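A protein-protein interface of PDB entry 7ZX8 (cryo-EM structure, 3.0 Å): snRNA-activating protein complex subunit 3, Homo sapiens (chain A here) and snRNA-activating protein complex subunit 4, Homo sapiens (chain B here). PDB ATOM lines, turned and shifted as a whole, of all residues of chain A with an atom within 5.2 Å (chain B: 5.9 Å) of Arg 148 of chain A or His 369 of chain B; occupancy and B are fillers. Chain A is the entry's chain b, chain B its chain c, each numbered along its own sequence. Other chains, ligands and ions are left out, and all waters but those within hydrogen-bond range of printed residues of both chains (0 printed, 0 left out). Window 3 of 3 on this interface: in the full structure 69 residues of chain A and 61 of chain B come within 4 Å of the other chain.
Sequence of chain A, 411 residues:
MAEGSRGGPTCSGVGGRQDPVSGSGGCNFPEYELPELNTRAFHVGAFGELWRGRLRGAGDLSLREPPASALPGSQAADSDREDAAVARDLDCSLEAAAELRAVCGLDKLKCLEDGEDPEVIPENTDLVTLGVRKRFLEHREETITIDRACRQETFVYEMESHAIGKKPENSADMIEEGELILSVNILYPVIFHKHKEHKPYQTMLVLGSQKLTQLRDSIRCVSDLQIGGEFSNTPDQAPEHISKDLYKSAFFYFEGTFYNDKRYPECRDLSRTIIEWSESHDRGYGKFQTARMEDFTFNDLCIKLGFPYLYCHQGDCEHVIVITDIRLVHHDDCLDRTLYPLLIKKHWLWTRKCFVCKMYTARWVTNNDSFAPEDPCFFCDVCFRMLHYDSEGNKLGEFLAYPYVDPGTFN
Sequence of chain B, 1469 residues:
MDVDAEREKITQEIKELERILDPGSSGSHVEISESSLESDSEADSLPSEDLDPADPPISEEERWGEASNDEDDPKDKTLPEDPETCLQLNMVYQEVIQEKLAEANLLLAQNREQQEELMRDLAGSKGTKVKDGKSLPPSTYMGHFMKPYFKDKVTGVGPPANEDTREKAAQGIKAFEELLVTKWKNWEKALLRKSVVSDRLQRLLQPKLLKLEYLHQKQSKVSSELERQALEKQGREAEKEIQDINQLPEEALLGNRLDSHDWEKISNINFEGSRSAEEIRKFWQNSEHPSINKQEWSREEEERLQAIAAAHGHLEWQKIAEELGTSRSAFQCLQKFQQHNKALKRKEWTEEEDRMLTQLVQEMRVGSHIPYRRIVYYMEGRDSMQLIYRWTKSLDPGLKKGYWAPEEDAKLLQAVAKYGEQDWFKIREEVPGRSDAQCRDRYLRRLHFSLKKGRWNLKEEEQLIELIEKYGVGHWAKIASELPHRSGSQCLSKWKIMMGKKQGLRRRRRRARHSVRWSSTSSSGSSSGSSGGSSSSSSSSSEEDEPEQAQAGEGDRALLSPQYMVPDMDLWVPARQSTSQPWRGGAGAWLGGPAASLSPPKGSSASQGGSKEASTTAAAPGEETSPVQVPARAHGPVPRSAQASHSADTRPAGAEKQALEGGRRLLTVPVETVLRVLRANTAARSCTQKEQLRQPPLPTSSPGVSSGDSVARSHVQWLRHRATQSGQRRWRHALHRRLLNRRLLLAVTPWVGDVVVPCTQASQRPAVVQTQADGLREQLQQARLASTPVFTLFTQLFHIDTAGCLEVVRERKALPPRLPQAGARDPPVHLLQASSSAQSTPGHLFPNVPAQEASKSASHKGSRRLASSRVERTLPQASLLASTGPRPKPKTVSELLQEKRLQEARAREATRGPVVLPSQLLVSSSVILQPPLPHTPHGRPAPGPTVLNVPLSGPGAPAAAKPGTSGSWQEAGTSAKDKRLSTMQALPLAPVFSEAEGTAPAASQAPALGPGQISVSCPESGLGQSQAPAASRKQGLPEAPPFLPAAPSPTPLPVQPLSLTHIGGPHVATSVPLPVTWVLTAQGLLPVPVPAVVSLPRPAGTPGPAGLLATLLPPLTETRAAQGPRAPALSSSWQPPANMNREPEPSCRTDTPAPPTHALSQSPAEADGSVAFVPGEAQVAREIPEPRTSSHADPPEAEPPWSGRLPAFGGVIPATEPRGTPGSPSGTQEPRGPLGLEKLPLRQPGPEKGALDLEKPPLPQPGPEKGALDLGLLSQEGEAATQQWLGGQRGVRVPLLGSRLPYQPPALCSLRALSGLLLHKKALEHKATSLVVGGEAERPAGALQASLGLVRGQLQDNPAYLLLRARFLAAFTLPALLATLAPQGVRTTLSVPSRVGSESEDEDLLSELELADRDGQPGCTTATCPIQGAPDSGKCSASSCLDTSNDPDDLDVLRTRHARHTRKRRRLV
The side-chain hydroxyl (OG1) of Thr 154 of chain A lies close to the backbone carbonyl oxygen (O) of Cys 150 of chain A, 3.5 Å away. OG1 of Thr 154 of chain A lies within hydrogen-bond range of O of Arg 151 of chain A (3.1 Å). The backbone carbonyl oxygen of Gly 367 of chain B lies within hydrogen-bond range of the guanidinium group of Arg 365 of chain B.
The side-chain hydroxyl (OG1) of Thr 154 of chain A lies close to a ring nitrogen (ND1) of His 369 of chain B. The side-chain carboxylate of Glu 158 of chain A lies close to the backbone carbonyl oxygen of Val 366 of chain B (2.9 Å). OE2 of Glu 158 of chain A lies close to N of Ser 368 of chain B, 2.3 Å away.
Of the 8 printed residues of chain B, 4 touch a printed residue of chain A. Hydrophobic or aromatic side chains of chain B within 4 Å of the printed part of chain A: His 369. Along chain B the printed residues that touch a printed residue of chain A span positions 366 to 369. Of the 8 printed residues of chain A, 4 touch a printed residue of chain B. Printed residues of chain A that touch a printed residue of chain B: Arg 148, Arg 151, Thr 154 and Glu 158. Among the printed residues, 6 pairs touch across the chains. Among the printed residues, no Asp or Glu carboxylate lies within 4 Å of a Lys or Arg side-chain nitrogen of the other chain.
His 369 of chain B touches just these residues of chain A: Arg 148, Arg 151 and Thr 154. Printed residues of chain A within 4 Å of Val 366 of chain B: Glu 158. Of the printed residues of chain A, Ser 368 of chain B touches Glu 158 (2.3 Å). Of the printed residues of chain B, Glu 158 of chain A touches Val 366, Gly 367 and Ser 368. Of the printed residues of chain B, Thr 154 of chain A touches His 369 (3.0 Å). Arg 365 of chain B touches none of the printed residues of chain A. Tyr 372 of chain B touches none of the printed residues of chain A. The nearest printed residue of chain A that does not touch Val 366 of chain B is Thr 154 of chain A (6.1 Å).
Among the printed residues, merely in contact across the chains: Glu 158 of chain A with Gly 367 of chain B, Arg 148 of chain A with His 369 of chain B and Arg 151 of chain A with His 369 of chain B.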
ATOM      1  N   ILE A 146      -1.392   5.182   2.672  1.00  0.00           N
ATOM      2  CA  ILE A 146      -1.889   6.160   1.711  1.00  0.00           C
ATOM      3  C   ILE A 146      -3.242   5.755   1.128  1.00  0.00           C
ATOM      4  O   ILE A 146      -3.303   4.991   0.159  1.00  0.00           O
ATOM      5  CB  ILE A 146      -0.843   6.444   0.612  1.00  0.00           C
ATOM      6  CG1 ILE A 146      -1.323   7.570  -0.308  1.00  0.00           C
ATOM      7  CG2 ILE A 146      -0.400   5.174  -0.123  1.00  0.00           C
ATOM      8  CD1 ILE A 146      -1.491   8.900   0.398  1.00  0.00           C
ATOM      9  N   ASP A 147      -4.335   6.251   1.704  1.00  0.00           N
ATOM     10  CA  ASP A 147      -5.699   5.871   1.326  1.00  0.00           C
ATOM     11  C   ASP A 147      -5.976   6.348  -0.097  1.00  0.00           C
ATOM     12  O   ASP A 147      -6.918   5.824  -0.715  1.00  0.00           O
ATOM     13  CB  ASP A 147      -6.653   6.402   2.398  1.00  0.00           C
ATOM     14  CG  ASP A 147      -8.028   5.775   2.316  1.00  0.00           C
ATOM     15  OD1 ASP A 147      -8.223   4.861   1.485  1.00  0.00           O
ATOM     16  OD2 ASP A 147      -8.923   6.197   3.079  1.00  0.00           O
ATOM     17  N   ARG A 148      -5.230   7.318  -0.635  1.00  0.00           N
ATOM     18  CA  ARG A 148      -5.492   7.910  -1.944  1.00  0.00           C
ATOM     19  C   ARG A 148      -5.850   6.863  -2.990  1.00  0.00           C
ATOM     20  O   ARG A 148      -5.217   5.805  -3.063  1.00  0.00           O
ATOM     21  CB  ARG A 148      -4.276   8.720  -2.402  1.00  0.00           C
ATOM     22  CG  ARG A 148      -4.601   9.850  -3.361  1.00  0.00           C
ATOM     23  CD  ARG A 148      -4.349   9.439  -4.795  1.00  0.00           C
ATOM     24  NE  ARG A 148      -3.069   8.752  -4.940  1.00  0.00           N
ATOM     25  CZ  ARG A 148      -2.719   8.051  -6.010  1.00  0.00           C
ATOM     26  NH1 ARG A 148      -3.552   7.943  -7.036  1.00  0.00           N
ATOM     27  NH2 ARG A 148      -1.532   7.461  -6.057  1.00  0.00           N
ATOM     28  N   ALA A 149      -6.877   7.141  -3.786  1.00  0.00           N
ATOM     29  CA  ALA A 149      -7.412   6.200  -4.756  1.00  0.00           C
ATOM     30  C   ALA A 149      -6.362   5.860  -5.806  1.00  0.00           C
ATOM     31  O   ALA A 149      -5.573   6.720  -6.209  1.00  0.00           O
ATOM     32  CB  ALA A 149      -8.658   6.767  -5.438  1.00  0.00           C
ATOM     33  N   CYS A 150      -6.360   4.601  -6.242  1.00  0.00           N
ATOM     34  CA  CYS A 150      -5.385   4.143  -7.220  1.00  0.00           C
ATOM     35  C   CYS A 150      -5.560   4.867  -8.546  1.00  0.00           C
ATOM     36  O   CYS A 150      -6.676   5.208  -8.941  1.00  0.00           O
ATOM     37  CB  CYS A 150      -5.518   2.639  -7.440  1.00  0.00           C
ATOM     38  SG  CYS A 150      -4.611   2.052  -8.880  1.00  0.00           S
ATOM     39  N   ARG A 151      -4.449   5.082  -9.245  1.00  0.00           N
ATOM     40  CA  ARG A 151      -4.510   5.831 -10.491  1.00  0.00           C
ATOM     41  C   ARG A 151      -5.130   5.041 -11.629  1.00  0.00           C
ATOM     42  O   ARG A 151      -5.440   5.633 -12.669  1.00  0.00           O
ATOM     43  CB  ARG A 151      -3.114   6.308 -10.891  1.00  0.00           C
ATOM     44  CG  ARG A 151      -2.048   5.243 -10.868  1.00  0.00           C
ATOM     45  CD  ARG A 151      -1.812   4.677 -12.251  1.00  0.00           C
ATOM     46  NE  ARG A 151      -0.572   3.917 -12.318  1.00  0.00           N
ATOM     47  CZ  ARG A 151      -0.226   3.144 -13.338  1.00  0.00           C
ATOM     48  NH1 ARG A 151      -1.030   3.021 -14.382  1.00  0.00           N
ATOM     49  NH2 ARG A 151       0.922   2.489 -13.310  1.00  0.00           N
ATOM     50  N   THR A 154      -9.244   5.423 -10.928  1.00  0.00           N
ATOM     51  CA  THR A 154      -9.667   6.739 -11.382  1.00  0.00           C
ATOM     52  C   THR A 154      -9.715   6.812 -12.897  1.00  0.00           C
ATOM     53  O   THR A 154     -10.577   7.492 -13.455  1.00  0.00           O
ATOM     54  CB  THR A 154      -8.727   7.814 -10.850  1.00  0.00           C
ATOM     55  OG1 THR A 154      -7.413   7.583 -11.364  1.00  0.00           O
ATOM     56  CG2 THR A 154      -8.679   7.770  -9.342  1.00  0.00           C
ATOM     57  N   GLU A 158     -13.158   7.835 -14.634  1.00  0.00           N
ATOM     58  CA  GLU A 158     -13.285   9.050 -15.424  1.00  0.00           C
ATOM     59  C   GLU A 158     -13.631   8.746 -16.868  1.00  0.00           C
ATOM     60  O   GLU A 158     -14.430   9.466 -17.470  1.00  0.00           O
ATOM     61  CB  GLU A 158     -11.991   9.855 -15.348  1.00  0.00           C
ATOM     62  CG  GLU A 158     -11.661  10.342 -13.957  1.00  0.00           C
ATOM     63  CD  GLU A 158     -12.076  11.772 -13.729  1.00  0.00           C
ATOM     64  OE1 GLU A 158     -13.177  12.151 -14.176  1.00  0.00           O
ATOM     65  OE2 GLU A 158     -11.300  12.521 -13.098  1.00  0.00           O
ATOM     66  N   ARG B 365      -7.154  16.035 -20.941  1.00  0.00           N
ATOM     67  CA  ARG B 365      -7.806  15.923 -19.646  1.00  0.00           C
ATOM     68  C   ARG B 365      -8.826  14.793 -19.663  1.00  0.00           C
ATOM     69  O   ARG B 365      -9.387  14.462 -20.709  1.00  0.00           O
ATOM     70  CB  ARG B 365      -8.499  17.242 -19.295  1.00  0.00           C
ATOM     71  CG  ARG B 365      -8.859  17.399 -17.830  1.00  0.00           C
ATOM     72  CD  ARG B 365      -7.606  17.388 -17.002  1.00  0.00           C
ATOM     73  NE  ARG B 365      -7.838  17.619 -15.582  1.00  0.00           N
ATOM     74  CZ  ARG B 365      -7.826  18.815 -15.011  1.00  0.00           C
ATOM     75  NH1 ARG B 365      -7.599  19.897 -15.739  1.00  0.00           N
ATOM     76  NH2 ARG B 365      -8.040  18.930 -13.709  1.00  0.00           N
ATOM     77  N   VAL B 366      -9.050  14.190 -18.499  1.00  0.00           N
ATOM     78  CA  VAL B 366     -10.181  13.297 -18.292  1.00  0.00           C
ATOM     79  C   VAL B 366     -10.949  13.617 -17.024  1.00  0.00           C
ATOM     80  O   VAL B 366     -11.758  12.787 -16.584  1.00  0.00           O
ATOM     81  CB  VAL B 366      -9.743  11.819 -18.281  1.00  0.00           C
ATOM     82  CG1 VAL B 366      -9.475  11.343 -19.691  1.00  0.00           C
ATOM     83  CG2 VAL B 366      -8.514  11.636 -17.404  1.00  0.00           C
ATOM     84  N   GLY B 367     -10.731  14.779 -16.423  1.00  0.00           N
ATOM     85  CA  GLY B 367     -11.186  15.021 -15.074  1.00  0.00           C
ATOM     86  C   GLY B 367      -9.973  15.166 -14.185  1.00  0.00           C
ATOM     87  O   GLY B 367      -9.267  16.177 -14.245  1.00  0.00           O
ATOM     88  N   SER B 368      -9.719  14.164 -13.356  1.00  0.00           N
ATOM     89  CA  SER B 368      -8.437  14.079 -12.681  1.00  0.00           C
ATOM     90  C   SER B 368      -7.592  12.980 -13.310  1.00  0.00           C
ATOM     91  O   SER B 368      -8.010  12.312 -14.261  1.00  0.00           O
ATOM     92  CB  SER B 368      -8.622  13.814 -11.190  1.00  0.00           C
ATOM     93  OG  SER B 368      -7.455  14.176 -10.471  1.00  0.00           O
ATOM     94  N   HIS B 369      -6.389  12.804 -12.767  1.00  0.00           N
ATOM     95  CA  HIS B 369      -5.447  11.802 -13.253  1.00  0.00           C
ATOM     96  C   HIS B 369      -5.205  11.958 -14.747  1.00  0.00           C
ATOM     97  O   HIS B 369      -5.606  11.118 -15.557  1.00  0.00           O
ATOM     98  CB  HIS B 369      -5.926  10.396 -12.899  1.00  0.00           C
ATOM     99  CG  HIS B 369      -5.692  10.043 -11.462  1.00  0.00           C
ATOM    100  ND1 HIS B 369      -4.544   9.418 -11.028  1.00  0.00           N
ATOM    101  CD2 HIS B 369      -6.443  10.260 -10.357  1.00  0.00           C
ATOM    102  CE1 HIS B 369      -4.606   9.248  -9.719  1.00  0.00           C
ATOM    103  NE2 HIS B 369      -5.750   9.750  -9.288  1.00  0.00           N
ATOM    104  N   ILE B 370      -4.588  13.074 -15.098  1.00  0.00           N
ATOM    105  CA  ILE B 370      -4.097  13.321 -16.454  1.00  0.00           C
ATOM    106  C   ILE B 370      -2.965  12.348 -16.763  1.00  0.00           C
ATOM    107  O   ILE B 370      -2.053  12.181 -15.934  1.00  0.00           O
ATOM    108  CB  ILE B 370      -3.626  14.761 -16.571  1.00  0.00           C
ATOM    109  CG1 ILE B 370      -2.693  15.084 -15.410  1.00  0.00           C
ATOM    110  CG2 ILE B 370      -4.786  15.681 -16.503  1.00  0.00           C
ATOM    111  CD1 ILE B 370      -2.299  16.527 -15.333  1.00  0.00           C
ATOM    112  N   PRO B 371      -2.966  11.687 -17.917  1.00  0.00           N
ATOM    113  CA  PRO B 371      -1.838  10.812 -18.243  1.00  0.00           C
ATOM    114  C   PRO B 371      -0.582  11.622 -18.480  1.00  0.00           C
ATOM    115  O   PRO B 371      -0.472  12.324 -19.487  1.00  0.00           O
ATOM    116  CB  PRO B 371      -2.304  10.097 -19.516  1.00  0.00           C
ATOM    117  CG  PRO B 371      -3.294  11.015 -20.118  1.00  0.00           C
ATOM    118  CD  PRO B 371      -3.985  11.691 -18.974  1.00  0.00           C
ATOM    119  N   TYR B 372       0.373  11.546 -17.553  1.00  0.00           N
ATOM    120  CA  TYR B 372       1.574  12.359 -17.692  1.00  0.00           C
ATOM    121  C   TYR B 372       2.527  11.783 -18.725  1.00  0.00           C
ATOM    122  O   TYR B 372       3.308  12.529 -19.319  1.00  0.00           O
ATOM    123  CB  TYR B 372       2.284  12.493 -16.353  1.00  0.00           C
ATOM    124  CG  TYR B 372       1.690  13.539 -15.454  1.00  0.00           C
ATOM    125  CD1 TYR B 372       0.647  13.235 -14.603  1.00  0.00           C
ATOM    126  CD2 TYR B 372       2.166  14.835 -15.472  1.00  0.00           C
ATOM    127  CE1 TYR B 372       0.108  14.186 -13.786  1.00  0.00           C
ATOM    128  CE2 TYR B 372       1.632  15.794 -14.660  1.00  0.00           C
ATOM    129  CZ  TYR B 372       0.602  15.463 -13.820  1.00  0.00           C
ATOM    130  OH  TYR B 372       0.062  16.420 -13.002  1.00  0.00           O
